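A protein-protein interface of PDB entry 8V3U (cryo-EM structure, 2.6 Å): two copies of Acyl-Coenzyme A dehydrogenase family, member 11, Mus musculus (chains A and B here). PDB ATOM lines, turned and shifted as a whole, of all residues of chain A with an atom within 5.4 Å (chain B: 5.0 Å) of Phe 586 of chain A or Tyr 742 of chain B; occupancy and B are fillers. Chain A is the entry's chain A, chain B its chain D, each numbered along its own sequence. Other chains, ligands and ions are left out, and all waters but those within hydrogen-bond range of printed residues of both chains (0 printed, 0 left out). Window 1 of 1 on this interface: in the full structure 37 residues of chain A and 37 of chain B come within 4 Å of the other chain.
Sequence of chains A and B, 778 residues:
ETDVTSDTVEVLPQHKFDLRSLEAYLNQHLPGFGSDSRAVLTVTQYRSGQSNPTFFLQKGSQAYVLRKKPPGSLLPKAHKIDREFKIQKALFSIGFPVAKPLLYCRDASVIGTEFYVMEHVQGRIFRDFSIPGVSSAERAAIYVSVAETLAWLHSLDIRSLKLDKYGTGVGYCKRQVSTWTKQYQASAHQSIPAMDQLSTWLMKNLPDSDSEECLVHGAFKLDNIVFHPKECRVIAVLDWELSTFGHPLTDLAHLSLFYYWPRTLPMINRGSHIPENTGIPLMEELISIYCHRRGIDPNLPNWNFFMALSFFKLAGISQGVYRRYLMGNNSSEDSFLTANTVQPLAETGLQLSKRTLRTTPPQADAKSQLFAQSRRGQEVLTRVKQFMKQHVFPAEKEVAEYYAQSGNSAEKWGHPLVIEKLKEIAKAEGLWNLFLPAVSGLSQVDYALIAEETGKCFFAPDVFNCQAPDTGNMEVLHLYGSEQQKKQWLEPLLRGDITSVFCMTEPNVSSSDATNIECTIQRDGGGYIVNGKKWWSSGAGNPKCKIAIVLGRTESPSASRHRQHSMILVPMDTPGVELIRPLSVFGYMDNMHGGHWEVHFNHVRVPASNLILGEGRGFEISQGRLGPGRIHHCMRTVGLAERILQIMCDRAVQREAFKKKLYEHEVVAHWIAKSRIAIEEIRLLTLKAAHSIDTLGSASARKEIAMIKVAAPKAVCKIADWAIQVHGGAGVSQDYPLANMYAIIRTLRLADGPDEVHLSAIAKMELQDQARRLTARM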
ATOM      1  N   SER A 584      19.118 -12.338  -1.068  1.00  0.00           N
ATOM      2  CA  SER A 584      19.332 -10.903  -0.984  1.00  0.00           C
ATOM      3  C   SER A 584      19.660 -10.324  -2.354  1.00  0.00           C
ATOM      4  O   SER A 584      20.190 -11.010  -3.231  1.00  0.00           O
ATOM      5  CB  SER A 584      20.458 -10.579  -0.002  1.00  0.00           C
ATOM      6  OG  SER A 584      21.701 -10.467  -0.670  1.00  0.00           O
ATOM      7  N   VAL A 585      19.332  -9.047  -2.529  1.00  0.00           N
ATOM      8  CA  VAL A 585      19.626  -8.305  -3.748  1.00  0.00           C
ATOM      9  C   VAL A 585      20.500  -7.124  -3.355  1.00  0.00           C
ATOM     10  O   VAL A 585      20.011  -6.152  -2.765  1.00  0.00           O
ATOM     11  CB  VAL A 585      18.351  -7.838  -4.461  1.00  0.00           C
ATOM     12  CG1 VAL A 585      18.685  -6.801  -5.514  1.00  0.00           C
ATOM     13  CG2 VAL A 585      17.624  -9.017  -5.081  1.00  0.00           C
ATOM     14  N   PHE A 586      21.795  -7.211  -3.667  1.00  0.00           N
ATOM     15  CA  PHE A 586      22.764  -6.161  -3.345  1.00  0.00           C
ATOM     16  C   PHE A 586      22.762  -5.826  -1.857  1.00  0.00           C
ATOM     17  O   PHE A 586      23.028  -4.692  -1.467  1.00  0.00           O
ATOM     18  CB  PHE A 586      22.511  -4.894  -4.167  1.00  0.00           C
ATOM     19  CG  PHE A 586      23.072  -4.945  -5.556  1.00  0.00           C
ATOM     20  CD1 PHE A 586      24.435  -4.846  -5.769  1.00  0.00           C
ATOM     21  CD2 PHE A 586      22.237  -5.086  -6.649  1.00  0.00           C
ATOM     22  CE1 PHE A 586      24.951  -4.892  -7.047  1.00  0.00           C
ATOM     23  CE2 PHE A 586      22.748  -5.132  -7.926  1.00  0.00           C
ATOM     24  CZ  PHE A 586      24.107  -5.035  -8.126  1.00  0.00           C
ATOM     25  N   GLY A 587      22.469  -6.803  -1.010  1.00  0.00           N
ATOM     26  CA  GLY A 587      22.365  -6.546   0.410  1.00  0.00           C
ATOM     27  C   GLY A 587      21.005  -6.088   0.889  1.00  0.00           C
ATOM     28  O   GLY A 587      20.869  -5.743   2.068  1.00  0.00           O
ATOM     29  N   TYR A 588      20.002  -6.064   0.019  1.00  0.00           N
ATOM     30  CA  TYR A 588      18.628  -5.758   0.388  1.00  0.00           C
ATOM     31  C   TYR A 588      17.827  -7.051   0.396  1.00  0.00           C
ATOM     32  O   TYR A 588      17.918  -7.843  -0.546  1.00  0.00           O
ATOM     33  CB  TYR A 588      18.000  -4.760  -0.586  1.00  0.00           C
ATOM     34  CG  TYR A 588      18.641  -3.393  -0.613  1.00  0.00           C
ATOM     35  CD1 TYR A 588      18.458  -2.499   0.430  1.00  0.00           C
ATOM     36  CD2 TYR A 588      19.414  -2.991  -1.692  1.00  0.00           C
ATOM     37  CE1 TYR A 588      19.035  -1.248   0.402  1.00  0.00           C
ATOM     38  CE2 TYR A 588      19.994  -1.743  -1.729  1.00  0.00           C
ATOM     39  CZ  TYR A 588      19.801  -0.876  -0.680  1.00  0.00           C
ATOM     40  OH  TYR A 588      20.377   0.370  -0.710  1.00  0.00           O
ATOM     41  N   ASP A 721      21.839   5.775 -12.267  1.00  0.00           N
ATOM     42  CA  ASP A 721      23.266   5.970 -12.030  1.00  0.00           C
ATOM     43  C   ASP A 721      23.640   7.446 -12.096  1.00  0.00           C
ATOM     44  O   ASP A 721      24.430   7.933 -11.276  1.00  0.00           O
ATOM     45  CB  ASP A 721      24.076   5.164 -13.043  1.00  0.00           C
ATOM     46  CG  ASP A 721      25.381   4.656 -12.472  1.00  0.00           C
ATOM     47  OD1 ASP A 721      26.433   4.865 -13.111  1.00  0.00           O
ATOM     48  OD2 ASP A 721      25.359   4.043 -11.385  1.00  0.00           O
ATOM     49  N   TYR A 742      18.176   1.790  -7.600  1.00  0.00           N
ATOM     50  CA  TYR A 742      19.118   1.252  -8.573  1.00  0.00           C
ATOM     51  C   TYR A 742      19.196  -0.263  -8.486  1.00  0.00           C
ATOM     52  O   TYR A 742      19.267  -0.941  -9.513  1.00  0.00           O
ATOM     53  CB  TYR A 742      20.510   1.857  -8.388  1.00  0.00           C
ATOM     54  CG  TYR A 742      21.539   1.175  -9.264  1.00  0.00           C
ATOM     55  CD1 TYR A 742      21.686   1.534 -10.596  1.00  0.00           C
ATOM     56  CD2 TYR A 742      22.341   0.152  -8.771  1.00  0.00           C
ATOM     57  CE1 TYR A 742      22.606   0.906 -11.406  1.00  0.00           C
ATOM     58  CE2 TYR A 742      23.261  -0.483  -9.576  1.00  0.00           C
ATOM     59  CZ  TYR A 742      23.391  -0.103 -10.891  1.00  0.00           C
ATOM     60  OH  TYR A 742      24.312  -0.731 -11.697  1.00  0.00           O
ATOM     61  N   ALA A 743      19.210  -0.812  -7.271  1.00  0.00           N
ATOM     62  CA  ALA A 743      19.269  -2.266  -7.128  1.00  0.00           C
ATOM     63  C   ALA A 743      18.052  -2.928  -7.765  1.00  0.00           C
ATOM     64  O   ALA A 743      18.176  -3.912  -8.511  1.00  0.00           O
ATOM     65  CB  ALA A 743      19.381  -2.641  -5.651  1.00  0.00           C
ATOM     66  N   ARG A 746      18.252  -2.705 -11.484  1.00  0.00           N
ATOM     67  CA  ARG A 746      19.302  -3.585 -11.978  1.00  0.00           C
ATOM     68  C   ARG A 746      18.818  -5.024 -12.055  1.00  0.00           C
ATOM     69  O   ARG A 746      19.189  -5.761 -12.974  1.00  0.00           O
ATOM     70  CB  ARG A 746      20.536  -3.468 -11.081  1.00  0.00           C
ATOM     71  CG  ARG A 746      21.714  -4.339 -11.481  1.00  0.00           C
ATOM     72  CD  ARG A 746      22.067  -4.177 -12.945  1.00  0.00           C
ATOM     73  NE  ARG A 746      23.226  -4.979 -13.317  1.00  0.00           N
ATOM     74  CZ  ARG A 746      23.176  -6.064 -14.079  1.00  0.00           C
ATOM     75  NH1 ARG A 746      22.031  -6.525 -14.551  1.00  0.00           N
ATOM     76  NH2 ARG A 746      24.304  -6.704 -14.370  1.00  0.00           N
ATOM     77  N   PHE B 586      24.819   0.891  -0.447  1.00  0.00           N
ATOM     78  CA  PHE B 586      23.944  -0.035  -1.168  1.00  0.00           C
ATOM     79  C   PHE B 586      23.384  -1.117  -0.251  1.00  0.00           C
ATOM     80  O   PHE B 586      23.128  -2.238  -0.682  1.00  0.00           O
ATOM     81  CB  PHE B 586      24.666  -0.679  -2.356  1.00  0.00           C
ATOM     82  CG  PHE B 586      24.714   0.184  -3.581  1.00  0.00           C
ATOM     83  CD1 PHE B 586      23.580   0.388  -4.344  1.00  0.00           C
ATOM     84  CD2 PHE B 586      25.897   0.786  -3.973  1.00  0.00           C
ATOM     85  CE1 PHE B 586      23.625   1.180  -5.472  1.00  0.00           C
ATOM     86  CE2 PHE B 586      25.946   1.577  -5.098  1.00  0.00           C
ATOM     87  CZ  PHE B 586      24.809   1.775  -5.849  1.00  0.00           C
ATOM     88  N   GLY B 587      23.183  -0.797   1.020  1.00  0.00           N
ATOM     89  CA  GLY B 587      22.734  -1.789   1.972  1.00  0.00           C
ATOM     90  C   GLY B 587      23.828  -2.601   2.630  1.00  0.00           C
ATOM     91  O   GLY B 587      23.516  -3.541   3.369  1.00  0.00           O
ATOM     92  N   TYR B 588      25.092  -2.277   2.382  1.00  0.00           N
ATOM     93  CA  TYR B 588      26.225  -2.905   3.047  1.00  0.00           C
ATOM     94  C   TYR B 588      26.784  -1.933   4.074  1.00  0.00           C
ATOM     95  O   TYR B 588      26.984  -0.754   3.769  1.00  0.00           O
ATOM     96  CB  TYR B 588      27.314  -3.289   2.045  1.00  0.00           C
ATOM     97  CG  TYR B 588      26.917  -4.332   1.027  1.00  0.00           C
ATOM     98  CD1 TYR B 588      26.772  -5.662   1.389  1.00  0.00           C
ATOM     99  CD2 TYR B 588      26.705  -3.987  -0.300  1.00  0.00           C
ATOM    100  CE1 TYR B 588      26.418  -6.616   0.460  1.00  0.00           C
ATOM    101  CE2 TYR B 588      26.352  -4.934  -1.235  1.00  0.00           C
ATOM    102  CZ  TYR B 588      26.211  -6.246  -0.850  1.00  0.00           C
ATOM    103  OH  TYR B 588      25.858  -7.194  -1.778  1.00  0.00           O
ATOM    104  N   CYS B 717      34.121  -1.003 -13.107  1.00  0.00           N
ATOM    105  CA  CYS B 717      32.670  -1.051 -12.949  1.00  0.00           C
ATOM    106  C   CYS B 717      32.011  -1.785 -14.108  1.00  0.00           C
ATOM    107  O   CYS B 717      31.106  -2.603 -13.902  1.00  0.00           O
ATOM    108  CB  CYS B 717      32.106   0.366 -12.837  1.00  0.00           C
ATOM    109  SG  CYS B 717      32.100   1.068 -11.176  1.00  0.00           S
ATOM    110  N   ALA B 720      32.705  -5.517 -13.714  1.00  0.00           N
ATOM    111  CA  ALA B 720      31.888  -6.109 -12.661  1.00  0.00           C
ATOM    112  C   ALA B 720      30.439  -6.271 -13.103  1.00  0.00           C
ATOM    113  O   ALA B 720      29.799  -7.284 -12.799  1.00  0.00           O
ATOM    114  CB  ALA B 720      31.969  -5.261 -11.392  1.00  0.00           C
ATOM    115  N   ASP B 721      29.902  -5.278 -13.815  1.00  0.00           N
ATOM    116  CA  ASP B 721      28.539  -5.388 -14.324  1.00  0.00           C
ATOM    117  C   ASP B 721      28.413  -6.535 -15.321  1.00  0.00           C
ATOM    118  O   ASP B 721      27.426  -7.283 -15.298  1.00  0.00           O
ATOM    119  CB  ASP B 721      28.114  -4.069 -14.965  1.00  0.00           C
ATOM    120  CG  ASP B 721      26.637  -3.790 -14.800  1.00  0.00           C
ATOM    121  OD1 ASP B 721      25.971  -3.487 -15.811  1.00  0.00           O
ATOM    122  OD2 ASP B 721      26.140  -3.869 -13.657  1.00  0.00           O
ATOM    123  N   ILE B 724      28.373  -9.788 -13.327  1.00  0.00           N
ATOM    124  CA  ILE B 724      27.080  -9.977 -12.675  1.00  0.00           C
ATOM    125  C   ILE B 724      26.040 -10.448 -13.683  1.00  0.00           C
ATOM    126  O   ILE B 724      25.250 -11.357 -13.403  1.00  0.00           O
ATOM    127  CB  ILE B 724      26.641  -8.683 -11.967  1.00  0.00           C
ATOM    128  CG1 ILE B 724      27.460  -8.462 -10.696  1.00  0.00           C
ATOM    129  CG2 ILE B 724      25.156  -8.722 -11.637  1.00  0.00           C
ATOM    130  CD1 ILE B 724      27.183  -7.144 -10.016  1.00  0.00           C
ATOM    131  N   VAL B 732      23.484 -11.199  -8.196  1.00  0.00           N
ATOM    132  CA  VAL B 732      23.122 -10.193  -7.202  1.00  0.00           C
ATOM    133  C   VAL B 732      22.940 -10.782  -5.810  1.00  0.00           C
ATOM    134  O   VAL B 732      22.799 -10.017  -4.843  1.00  0.00           O
ATOM    135  CB  VAL B 732      21.841  -9.432  -7.611  1.00  0.00           C
ATOM    136  CG1 VAL B 732      22.006  -8.811  -8.984  1.00  0.00           C
ATOM    137  CG2 VAL B 732      20.636 -10.357  -7.581  1.00  0.00           C
ATOM    138  N   LEU B 738      30.206 -10.860  -6.118  1.00  0.00           N
ATOM    139  CA  LEU B 738      30.174  -9.881  -7.197  1.00  0.00           C
ATOM    140  C   LEU B 738      29.372  -8.637  -6.832  1.00  0.00           C
ATOM    141  O   LEU B 738      29.716  -7.537  -7.272  1.00  0.00           O
ATOM    142  CB  LEU B 738      29.609 -10.518  -8.465  1.00  0.00           C
ATOM    143  CG  LEU B 738      30.437 -11.638  -9.095  1.00  0.00           C
ATOM    144  CD1 LEU B 738      29.633 -12.345 -10.166  1.00  0.00           C
ATOM    145  CD2 LEU B 738      31.736 -11.094  -9.664  1.00  0.00           C
ATOM    146  N   ALA B 739      28.304  -8.783  -6.045  1.00  0.00           N
ATOM    147  CA  ALA B 739      27.465  -7.632  -5.719  1.00  0.00           C
ATOM    148  C   ALA B 739      28.185  -6.670  -4.780  1.00  0.00           C
ATOM    149  O   ALA B 739      28.179  -5.450  -4.995  1.00  0.00           O
ATOM    150  CB  ALA B 739      26.146  -8.104  -5.109  1.00  0.00           C
ATOM    151  N   ASN B 740      28.805  -7.201  -3.724  1.00  0.00           N
ATOM    152  CA  ASN B 740      29.590  -6.360  -2.827  1.00  0.00           C
ATOM    153  C   ASN B 740      30.772  -5.741  -3.561  1.00  0.00           C
ATOM    154  O   ASN B 740      31.119  -4.574  -3.333  1.00  0.00           O
ATOM    155  CB  ASN B 740      30.061  -7.180  -1.628  1.00  0.00           C
ATOM    156  CG  ASN B 740      30.331  -6.328  -0.411  1.00  0.00           C
ATOM    157  OD1 ASN B 740      30.208  -5.105  -0.456  1.00  0.00           O
ATOM    158  ND2 ASN B 740      30.692  -6.968   0.690  1.00  0.00           N
ATOM    159  N   MET B 741      31.400  -6.516  -4.447  1.00  0.00           N
ATOM    160  CA  MET B 741      32.474  -5.989  -5.280  1.00  0.00           C
ATOM    161  C   MET B 741      31.991  -4.801  -6.100  1.00  0.00           C
ATOM    162  O   MET B 741      32.659  -3.762  -6.162  1.00  0.00           O
ATOM    163  CB  MET B 741      33.001  -7.091  -6.197  1.00  0.00           C
ATOM    164  CG  MET B 741      34.311  -7.703  -5.762  1.00  0.00           C
ATOM    165  SD  MET B 741      34.540  -9.365  -6.420  1.00  0.00           S
ATOM    166  CE  MET B 741      35.466 -10.127  -5.093  1.00  0.00           C
ATOM    167  N   TYR B 742      30.824  -4.937  -6.736  1.00  0.00           N
ATOM    168  CA  TYR B 742      30.298  -3.847  -7.546  1.00  0.00           C
ATOM    169  C   TYR B 742      30.002  -2.622  -6.697  1.00  0.00           C
ATOM    170  O   TYR B 742      30.268  -1.495  -7.118  1.00  0.00           O
ATOM    171  CB  TYR B 742      29.038  -4.275  -8.300  1.00  0.00           C
ATOM    172  CG  TYR B 742      28.377  -3.105  -8.997  1.00  0.00           C
ATOM    173  CD1 TYR B 742      28.829  -2.667 -10.233  1.00  0.00           C
ATOM    174  CD2 TYR B 742      27.322  -2.418  -8.407  1.00  0.00           C
ATOM    175  CE1 TYR B 742      28.246  -1.591 -10.865  1.00  0.00           C
ATOM    176  CE2 TYR B 742      26.736  -1.339  -9.030  1.00  0.00           C
ATOM    177  CZ  TYR B 742      27.199  -0.930 -10.259  1.00  0.00           C
ATOM    178  OH  TYR B 742      26.613   0.143 -10.889  1.00  0.00           O
ATOM    179  N   ALA B 743      29.427  -2.818  -5.509  1.00  0.00           N
ATOM    180  CA  ALA B 743      29.132  -1.678  -4.644  1.00  0.00           C
ATOM    181  C   ALA B 743      30.409  -0.935  -4.263  1.00  0.00           C
ATOM    182  O   ALA B 743      30.476   0.302  -4.334  1.00  0.00           O
ATOM    183  CB  ALA B 743      28.385  -2.148  -3.396  1.00  0.00           C
ATOM    184  N   ILE B 744      31.447  -1.686  -3.886  1.00  0.00           N
ATOM    185  CA  ILE B 744      32.706  -1.068  -3.480  1.00  0.00           C
ATOM    186  C   ILE B 744      33.348  -0.325  -4.647  1.00  0.00           C
ATOM    187  O   ILE B 744      33.847   0.794  -4.486  1.00  0.00           O
ATOM    188  CB  ILE B 744      33.649  -2.128  -2.882  1.00  0.00           C
ATOM    189  CG1 ILE B 744      33.082  -2.635  -1.556  1.00  0.00           C
ATOM    190  CG2 ILE B 744      35.040  -1.560  -2.680  1.00  0.00           C
ATOM    191  CD1 ILE B 744      33.643  -3.961  -1.117  1.00  0.00           C
ATOM    192  N   ILE B 745      33.343  -0.927  -5.839  1.00  0.00           N
ATOM    193  CA  ILE B 745      33.915  -0.243  -6.997  1.00  0.00           C
ATOM    194  C   ILE B 745      33.087   0.982  -7.371  1.00  0.00           C
ATOM    195  O   ILE B 745      33.634   2.000  -7.810  1.00  0.00           O
ATOM    196  CB  ILE B 745      34.055  -1.207  -8.190  1.00  0.00           C
ATOM    197  CG1 ILE B 745      34.894  -2.422  -7.806  1.00  0.00           C
ATOM    198  CG2 ILE B 745      34.704  -0.509  -9.369  1.00  0.00           C
ATOM    199  CD1 ILE B 745      34.616  -3.634  -8.661  1.00  0.00           C
ATOM    200  N   ARG B 746      31.765   0.909  -7.209  1.00  0.00           N
ATOM    201  CA  ARG B 746      30.904   2.040  -7.525  1.00  0.00           C
ATOM    202  C   ARG B 746      31.192   3.219  -6.609  1.00  0.00           C
ATOM    203  O   ARG B 746      31.136   4.376  -7.041  1.00  0.00           O
ATOM    204  CB  ARG B 746      29.438   1.615  -7.426  1.00  0.00           C
ATOM    205  CG  ARG B 746      28.423   2.704  -7.730  1.00  0.00           C
ATOM    206  CD  ARG B 746      28.718   3.403  -9.041  1.00  0.00           C
ATOM    207  NE  ARG B 746      27.719   4.418  -9.353  1.00  0.00           N
ATOM    208  CZ  ARG B 746      27.936   5.725  -9.310  1.00  0.00           C
ATOM    209  NH1 ARG B 746      29.107   6.220  -8.945  1.00  0.00           N
ATOM    210  NH2 ARG B 746      26.952   6.557  -9.637  1.00  0.00           N
ATOM    211  N   THR B 747      31.506   2.951  -5.341  1.00  0.00           N
ATOM    212  CA  THR B 747      31.889   4.051  -4.462  1.00  0.00           C
ATOM    213  C   THR B 747      33.254   4.639  -4.797  1.00  0.00           C
ATOM    214  O   THR B 747      33.592   5.703  -4.270  1.00  0.00           O
ATOM    215  CB  THR B 747      31.878   3.600  -3.006  1.00  0.00           C
ATOM    216  OG1 THR B 747      32.641   2.395  -2.869  1.00  0.00           O
ATOM    217  CG2 THR B 747      30.463   3.362  -2.550  1.00  0.00           C
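Phe 586 of chain A touches just these residues of chain B: Phe 586 (2.6 Å), Tyr 588 (3.3 Å), Val 732 (3.2 Å), Ala 739 (3.7 Å) and Tyr 742 (3.7 Å). Of the printed residues of chain A, Arg 746 of chain B touches Asp 721. Of the printed residues of chain B, Asp 721 of chain A touches Arg 746. Of the printed residues of chain B, Arg 746 of chain A touches Asp 721 (3.1 Å) and Ile 724 (3.5 Å). Of the printed residues of chain B, Tyr 742 of chain A touches Phe 586 (3.7 Å) and Tyr 742 (2.6 Å). The nearest printed residue of chain A that does not touch Phe 586 of chain B is Gly 587 of chain A (4.5 Å).
CA of Val 585 of chain A touches O of Val 732 of chain B, 3.8 Å away. CE2 of Tyr 588 of chain B touches O of Phe 586 of chain A, 3.3 Å away. CD1 of Phe 586 of chain A touches CB of Ala 739 of chain B (3.7 Å). Phe 586 of chain A touches Tyr 742 of chain B (CE1 to CD2, 3.7 Å). Gly 587 of chain A touches Gly 587 of chain B. CE2 of Tyr 588 of chain A touches O of Phe 586 of chain B, 3.3 Å away. Tyr 742 of chain A touches Phe 586 of chain B. CG2 of Ile 724 of chain B touches NH2 of Arg 746 of chain A, at 3.5 Å.
Phe 586 of chain A touches Tyr 588 of chain B, and with the chains exchanged Tyr 588 of chain A touches Phe 586 of chain B. Gly 587 of chain A touches its own counterpart, Gly 587 of chain B. Gly 587 of chain A touches Tyr 588 of chain B, and with the chains exchanged Tyr 588 of chain A touches Gly 587 of chain B. Tyr 742 of chain B touches its own counterpart, Tyr 742 of chain A. Positions printed for both chains: 586, 587, 588, 721, 742, 743 and 746. Of the 16 pairs that touch across the chains among the printed residues, 11 have their exchanged pair printed and touching as well.
NE of Arg 746 of chain A lies within salt-bridge range of OD2 of Asp 721 of chain B (3.1 Å). OH of Tyr 742 of chain A lies within hydrogen-bond range of OH of Tyr 742 of chain B, 2.6 Å away. The guanidinium group (NE) of Arg 746 of chain B is in salt-bridge range of the side-chain carboxylate (OD2) of Asp 721 of chain A. The side-chain hydroxyl (OH) of Tyr 588 of chain B is in hydrogen-bond range of the backbone NH (N) of Gly 587 of chain A, 3.5 Å away. The side-chain hydroxyl (OH) of Tyr 588 of chain A lies within hydrogen-bond range of the backbone NH (N) of Gly 587 of chain B (3.5 Å). O of Phe 586 of chain B lies close to O of Phe 586 of chain A, 2.6 Å away. The backbone carbonyl oxygen of Val 732 of chain B lies within hydrogen-bond range of the backbone NH of Phe 586 of chain A (3.2 Å). The backbone carbonyl oxygen of Val 732 of chain B sits close to the backbone carbonyl oxygen of Ser 584 of chain A, 3.2 Å away.
Of the 18 printed residues of chain B, 9 touch a printed residue of chain A. Of the 9 printed residues of chain A, 8 touch a printed residue of chain B. Hydrophobic or aromatic side chains of chain A that line the printed part of chain B: Phe 586, Tyr 588 and Tyr 742. Along chain A the printed residues that touch a printed residue of chain B span positions 584 to 746. Among the printed residues, Asp or Glu carboxylates within 4 Å of a Lys or Arg side-chain nitrogen of the other chain: Asp 721 of chain A with Arg 746 of chain B (3.1 Å) and Arg 746 of chain A with Asp 721 of chain B (3.1 Å).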
